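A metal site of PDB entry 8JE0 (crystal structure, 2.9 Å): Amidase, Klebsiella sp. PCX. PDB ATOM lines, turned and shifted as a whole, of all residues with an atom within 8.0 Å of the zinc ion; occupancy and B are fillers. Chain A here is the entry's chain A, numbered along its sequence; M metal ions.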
ATOM      1  N   HIS A  62      19.704   5.148   8.358  1.00  0.00           N
ATOM      2  CA  HIS A  62      19.293   4.164   9.360  1.00  0.00           C
ATOM      3  C   HIS A  62      20.553   3.692  10.068  1.00  0.00           C
ATOM      4  O   HIS A  62      21.266   2.810   9.568  1.00  0.00           O
ATOM      5  CB  HIS A  62      18.500   3.013   8.736  1.00  0.00           C
ATOM      6  CG  HIS A  62      18.079   1.963   9.717  1.00  0.00           C
ATOM      7  ND1 HIS A  62      16.901   1.259   9.595  1.00  0.00           N
ATOM      8  CD2 HIS A  62      18.673   1.487  10.841  1.00  0.00           C
ATOM      9  CE1 HIS A  62      16.793   0.399  10.600  1.00  0.00           C
ATOM     10  NE2 HIS A  62      17.856   0.518  11.361  1.00  0.00           N
ATOM     11  N   GLY A  63      20.851   4.303  11.212  1.00  0.00           N
ATOM     12  CA  GLY A  63      21.829   3.792  12.124  1.00  0.00           C
ATOM     13  C   GLY A  63      21.234   3.717  13.515  1.00  0.00           C
ATOM     14  O   GLY A  63      20.161   4.256  13.781  1.00  0.00           O
ATOM     15  N   HIS A  64      21.946   3.032  14.395  1.00  0.00           N
ATOM     16  CA  HIS A  64      21.529   2.900  15.779  1.00  0.00           C
ATOM     17  C   HIS A  64      22.661   3.462  16.634  1.00  0.00           C
ATOM     18  O   HIS A  64      23.747   2.877  16.688  1.00  0.00           O
ATOM     19  CB  HIS A  64      21.181   1.432  16.097  1.00  0.00           C
ATOM     20  CG  HIS A  64      20.076   0.877  15.244  1.00  0.00           C
ATOM     21  ND1 HIS A  64      18.800   1.389  15.256  1.00  0.00           N
ATOM     22  CD2 HIS A  64      20.065  -0.130  14.332  1.00  0.00           C
ATOM     23  CE1 HIS A  64      18.046   0.710  14.407  1.00  0.00           C
ATOM     24  NE2 HIS A  64      18.784  -0.218  13.829  1.00  0.00           N
ATOM     25  N   ILE A  72      23.280  -2.145  21.329  1.00  0.00           N
ATOM     26  CA  ILE A  72      23.627  -2.285  19.920  1.00  0.00           C
ATOM     27  C   ILE A  72      24.226  -1.033  19.297  1.00  0.00           C
ATOM     28  O   ILE A  72      24.773  -1.117  18.184  1.00  0.00           O
ATOM     29  CB  ILE A  72      22.392  -2.691  19.083  1.00  0.00           C
ATOM     30  CG1 ILE A  72      21.295  -1.642  19.245  1.00  0.00           C
ATOM     31  CG2 ILE A  72      21.904  -4.051  19.493  1.00  0.00           C
ATOM     32  CD1 ILE A  72      20.282  -1.642  18.124  1.00  0.00           C
ATOM     33  N   ASP A  90      18.748   8.138  13.710  1.00  0.00           N
ATOM     34  CA  ASP A  90      18.654   6.951  14.548  1.00  0.00           C
ATOM     35  C   ASP A  90      17.300   6.291  14.336  1.00  0.00           C
ATOM     36  O   ASP A  90      16.267   6.890  14.638  1.00  0.00           O
ATOM     37  CB  ASP A  90      18.855   7.325  16.017  1.00  0.00           C
ATOM     38  CG  ASP A  90      18.886   6.097  16.917  1.00  0.00           C
ATOM     39  OD1 ASP A  90      19.986   5.534  17.116  1.00  0.00           O
ATOM     40  OD2 ASP A  90      17.820   5.711  17.422  1.00  0.00           O
ATOM     41  N   ALA A  91      17.316   5.065  13.812  1.00  0.00           N
ATOM     42  CA  ALA A  91      16.078   4.364  13.465  1.00  0.00           C
ATOM     43  C   ALA A  91      15.454   3.694  14.690  1.00  0.00           C
ATOM     44  O   ALA A  91      15.336   2.477  14.796  1.00  0.00           O
ATOM     45  CB  ALA A  91      16.339   3.348  12.361  1.00  0.00           C
ATOM     46  N   GLY A  92      15.060   4.535  15.636  1.00  0.00           N
ATOM     47  CA  GLY A  92      14.204   4.096  16.725  1.00  0.00           C
ATOM     48  C   GLY A  92      14.856   3.267  17.802  1.00  0.00           C
ATOM     49  O   GLY A  92      14.239   2.323  18.305  1.00  0.00           O
ATOM     50  N   SER A  93      16.089   3.605  18.191  1.00  0.00           N
ATOM     51  CA  SER A  93      16.698   2.935  19.333  1.00  0.00           C
ATOM     52  C   SER A  93      16.017   3.351  20.629  1.00  0.00           C
ATOM     53  O   SER A  93      15.967   2.559  21.589  1.00  0.00           O
ATOM     54  CB  SER A  93      18.192   3.236  19.392  1.00  0.00           C
ATOM     55  OG  SER A  93      18.807   3.019  18.136  1.00  0.00           O
ATOM     56  N   LEU A 125      14.897  -0.175  21.467  1.00  0.00           N
ATOM     57  CA  LEU A 125      15.625  -1.387  21.136  1.00  0.00           C
ATOM     58  C   LEU A 125      16.701  -1.703  22.177  1.00  0.00           C
ATOM     59  O   LEU A 125      17.710  -2.341  21.854  1.00  0.00           O
ATOM     60  CB  LEU A 125      16.244  -1.268  19.741  1.00  0.00           C
ATOM     61  CG  LEU A 125      15.246  -0.854  18.654  1.00  0.00           C
ATOM     62  CD1 LEU A 125      15.951  -0.661  17.327  1.00  0.00           C
ATOM     63  CD2 LEU A 125      14.123  -1.867  18.543  1.00  0.00           C
ATOM     64  N   LEU A 128      17.983  -5.500  22.766  1.00  0.00           N
ATOM     65  CA  LEU A 128      18.285  -6.233  21.535  1.00  0.00           C
ATOM     66  C   LEU A 128      19.770  -6.500  21.338  1.00  0.00           C
ATOM     67  O   LEU A 128      20.218  -6.620  20.196  1.00  0.00           O
ATOM     68  CB  LEU A 128      17.730  -5.482  20.334  1.00  0.00           C
ATOM     69  CG  LEU A 128      16.274  -5.674  19.922  1.00  0.00           C
ATOM     70  CD1 LEU A 128      16.038  -4.892  18.656  1.00  0.00           C
ATOM     71  CD2 LEU A 128      15.968  -7.138  19.698  1.00  0.00           C
ATOM     72  N   LYS A 164       9.186   4.826  14.621  1.00  0.00           N
ATOM     73  CA  LYS A 164       9.814   3.618  14.103  1.00  0.00           C
ATOM     74  C   LYS A 164       9.097   2.388  14.645  1.00  0.00           C
ATOM     75  O   LYS A 164       8.831   2.289  15.846  1.00  0.00           O
ATOM     76  CB  LYS A 164      11.296   3.569  14.472  1.00  0.00           C
ATOM     77  CG  LYS A 164      11.930   2.188  14.250  1.00  0.00           C
ATOM     78  CD  LYS A 164      12.743   2.143  12.966  1.00  0.00           C
ATOM     79  CE  LYS A 164      13.123   0.710  12.589  1.00  0.00           C
ATOM     80  NZ  LYS A 164      14.441   0.254  13.131  1.00  0.00           N
ATOM     81  N   LEU A 165       8.785   1.457  13.741  1.00  0.00           N
ATOM     82  CA  LEU A 165       8.230   0.163  14.116  1.00  0.00           C
ATOM     83  C   LEU A 165       9.035  -0.929  13.435  1.00  0.00           C
ATOM     84  O   LEU A 165       9.373  -0.824  12.252  1.00  0.00           O
ATOM     85  CB  LEU A 165       6.759   0.044  13.721  1.00  0.00           C
ATOM     86  CG  LEU A 165       6.164  -1.351  13.907  1.00  0.00           C
ATOM     87  CD1 LEU A 165       5.975  -1.689  15.382  1.00  0.00           C
ATOM     88  CD2 LEU A 165       4.862  -1.509  13.143  1.00  0.00           C
ATOM     89  N   ARG A 166       9.337  -1.984  14.179  1.00  0.00           N
ATOM     90  CA  ARG A 166       9.877  -3.203  13.612  1.00  0.00           C
ATOM     91  C   ARG A 166       8.753  -4.221  13.525  1.00  0.00           C
ATOM     92  O   ARG A 166       8.085  -4.493  14.527  1.00  0.00           O
ATOM     93  CB  ARG A 166      11.048  -3.726  14.429  1.00  0.00           C
ATOM     94  CG  ARG A 166      12.336  -2.956  14.184  1.00  0.00           C
ATOM     95  CD  ARG A 166      13.322  -3.124  15.315  1.00  0.00           C
ATOM     96  NE  ARG A 166      14.334  -4.124  15.007  1.00  0.00           N
ATOM     97  CZ  ARG A 166      14.448  -5.290  15.624  1.00  0.00           C
ATOM     98  NH1 ARG A 166      13.594  -5.651  16.577  1.00  0.00           N
ATOM     99  NH2 ARG A 166      15.436  -6.116  15.292  1.00  0.00           N
ATOM    100  N   CYS A 197       8.401   4.808   9.958  1.00  0.00           N
ATOM    101  CA  CYS A 197       9.489   4.022   9.391  1.00  0.00           C
ATOM    102  C   CYS A 197       9.380   2.613   9.944  1.00  0.00           C
ATOM    103  O   CYS A 197       9.328   2.427  11.158  1.00  0.00           O
ATOM    104  CB  CYS A 197      10.845   4.639   9.745  1.00  0.00           C
ATOM    105  SG  CYS A 197      12.238   3.483   9.672  1.00  0.00           S
ATOM    106  N   HIS A 199      10.755  -1.441   9.783  1.00  0.00           N
ATOM    107  CA  HIS A 199      11.440  -2.676   9.410  1.00  0.00           C
ATOM    108  C   HIS A 199      10.419  -3.611   8.776  1.00  0.00           C
ATOM    109  O   HIS A 199       9.389  -3.920   9.391  1.00  0.00           O
ATOM    110  CB  HIS A 199      12.048  -3.341  10.657  1.00  0.00           C
ATOM    111  CG  HIS A 199      13.499  -3.059  10.891  1.00  0.00           C
ATOM    112  ND1 HIS A 199      14.410  -4.053  11.187  1.00  0.00           N
ATOM    113  CD2 HIS A 199      14.190  -1.893  10.984  1.00  0.00           C
ATOM    114  CE1 HIS A 199      15.595  -3.526  11.390  1.00  0.00           C
ATOM    115  NE2 HIS A 199      15.495  -2.213  11.281  1.00  0.00           N
ATOM    116  N   ALA A 221      11.836   0.447   5.259  1.00  0.00           N
ATOM    117  CA  ALA A 221      13.189   0.051   5.584  1.00  0.00           C
ATOM    118  C   ALA A 221      13.477  -1.379   5.144  1.00  0.00           C
ATOM    119  O   ALA A 221      12.613  -2.258   5.211  1.00  0.00           O
ATOM    120  CB  ALA A 221      13.460   0.195   7.083  1.00  0.00           C
ATOM    121  N   HIS A 222      14.708  -1.594   4.682  1.00  0.00           N
ATOM    122  CA  HIS A 222      15.195  -2.885   4.196  1.00  0.00           C
ATOM    123  C   HIS A 222      14.350  -3.367   3.008  1.00  0.00           C
ATOM    124  O   HIS A 222      13.666  -4.384   3.057  1.00  0.00           O
ATOM    125  CB  HIS A 222      15.210  -3.926   5.324  1.00  0.00           C
ATOM    126  CG  HIS A 222      15.735  -3.403   6.618  1.00  0.00           C
ATOM    127  ND1 HIS A 222      17.076  -3.440   6.958  1.00  0.00           N
ATOM    128  CD2 HIS A 222      15.093  -2.890   7.704  1.00  0.00           C
ATOM    129  CE1 HIS A 222      17.240  -2.947   8.170  1.00  0.00           C
ATOM    130  NE2 HIS A 222      16.059  -2.598   8.640  1.00  0.00           N
ATOM    131  N   SER A 255      18.400  -0.752   4.043  1.00  0.00           N
ATOM    132  CA  SER A 255      19.171  -0.783   5.282  1.00  0.00           C
ATOM    133  C   SER A 255      19.916  -2.100   5.339  1.00  0.00           C
ATOM    134  O   SER A 255      19.347  -3.146   5.664  1.00  0.00           O
ATOM    135  CB  SER A 255      18.260  -0.574   6.479  1.00  0.00           C
ATOM    136  OG  SER A 255      18.116   0.794   6.785  1.00  0.00           O
ATOM    137  N   GLY A 257      21.504  -4.569   6.813  1.00  0.00           N
ATOM    138  CA  GLY A 257      21.808  -5.152   8.103  1.00  0.00           C
ATOM    139  C   GLY A 257      22.806  -6.284   8.007  1.00  0.00           C
ATOM    140  O   GLY A 257      23.622  -6.324   7.080  1.00  0.00           O
ATOM    141  N   HIS A 260      19.408  -8.289   6.346  1.00  0.00           N
ATOM    142  CA  HIS A 260      18.401  -7.432   5.737  1.00  0.00           C
ATOM    143  C   HIS A 260      18.721  -7.067   4.290  1.00  0.00           C
ATOM    144  O   HIS A 260      18.177  -6.096   3.767  1.00  0.00           O
ATOM    145  CB  HIS A 260      18.233  -6.157   6.566  1.00  0.00           C
ATOM    146  CG  HIS A 260      17.770  -6.392   7.972  1.00  0.00           C
ATOM    147  ND1 HIS A 260      16.711  -7.203   8.272  1.00  0.00           N
ATOM    148  CD2 HIS A 260      18.237  -5.919   9.144  1.00  0.00           C
ATOM    149  CE1 HIS A 260      16.527  -7.230   9.584  1.00  0.00           C
ATOM    150  NE2 HIS A 260      17.443  -6.453  10.142  1.00  0.00           N
ATOM    151  N   THR A 281      23.009   1.803   6.516  1.00  0.00           N
ATOM    152  CA  THR A 281      23.794   0.703   7.061  1.00  0.00           C
ATOM    153  C   THR A 281      23.045  -0.175   8.051  1.00  0.00           C
ATOM    154  O   THR A 281      23.412  -1.343   8.191  1.00  0.00           O
ATOM    155  CB  THR A 281      25.052   1.243   7.769  1.00  0.00           C
ATOM    156  OG1 THR A 281      24.666   2.245   8.715  1.00  0.00           O
ATOM    157  CG2 THR A 281      26.000   1.859   6.764  1.00  0.00           C
ATOM    158  N   ASP A 282      22.014   0.328   8.726  1.00  0.00           N
ATOM    159  CA  ASP A 282      21.525  -0.305   9.960  1.00  0.00           C
ATOM    160  C   ASP A 282      22.697  -0.539  10.905  1.00  0.00           C
ATOM    161  O   ASP A 282      22.865  -1.606  11.495  1.00  0.00           O
ATOM    162  CB  ASP A 282      20.769  -1.611   9.658  1.00  0.00           C
ATOM    163  CG  ASP A 282      19.943  -2.104  10.857  1.00  0.00           C
ATOM    164  OD1 ASP A 282      19.280  -1.288  11.537  1.00  0.00           O
ATOM    165  OD2 ASP A 282      19.939  -3.336  11.096  1.00  0.00           O
ATOM    166  N   LEU A 283      23.541   0.498  11.011  1.00  0.00           N
ATOM    167  CA  LEU A 283      24.772   0.433  11.783  1.00  0.00           C
ATOM    168  C   LEU A 283      24.504   0.016  13.226  1.00  0.00           C
ATOM    169  O   LEU A 283      23.721   0.654  13.926  1.00  0.00           O
ATOM    170  CB  LEU A 283      25.481   1.778  11.752  1.00  0.00           C
ATOM    171  CG  LEU A 283      26.977   1.771  12.075  1.00  0.00           C
ATOM    172  CD1 LEU A 283      27.770   0.932  11.078  1.00  0.00           C
ATOM    173  CD2 LEU A 283      27.519   3.193  12.125  1.00  0.00           C
ATOM    174  N   THR A 284      25.153  -1.070  13.643  1.00  0.00           N
ATOM    175  CA  THR A 284      25.193  -1.496  15.027  1.00  0.00           C
ATOM    176  C   THR A 284      26.633  -1.791  15.405  1.00  0.00           C
ATOM    177  O   THR A 284      27.513  -1.891  14.547  1.00  0.00           O
ATOM    178  CB  THR A 284      24.327  -2.726  15.288  1.00  0.00           C
ATOM    179  OG1 THR A 284      24.982  -3.892  14.749  1.00  0.00           O
ATOM    180  CG2 THR A 284      22.938  -2.579  14.657  1.00  0.00           C
HETATM  181 ZN    ZN M   1      17.309  -1.410  12.485  1.00  0.00          ZN
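The side-chain hydroxyl of Ser 255 lies close to a ring nitrogen (ND1) of His 62, 3.1 Å away. NE2 of His 199 lies close to NZ of Lys 164, 3.3 Å away. A ring nitrogen (ND1) of His 199 sits close to a ring nitrogen (NE2) of His 222. N of His 199 lies within hydrogen-bond range of O of Leu 165, 2.9 Å away. O of Leu 283 sits at hydrogen-bond distance from N of His 64 (3.0 Å). ND1 of His 64 is in hydrogen-bond range of OG of Ser 93, at 3.3 Å. The side-chain amino group of Lys 164 lies within hydrogen-bond range of the backbone carbonyl oxygen of Ala 91 (2.9 Å).
Residues that only touch the zinc ion: Lys 164. Of the 24 residues printed, 5 come within 4 Å of the zinc ion. The nearest printed residue that does not touch the zinc ion is His 222 (4.2 Å).
The zinc ion is bound by the side-chain carboxylate (OD1) of Asp 282 (2.2 Å), a ring nitrogen (NE2) of His 62 (2.3 Å), a ring nitrogen (NE2) of His 199 (2.3 Å) and a ring nitrogen (NE2) of His 64 (2.3 Å).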
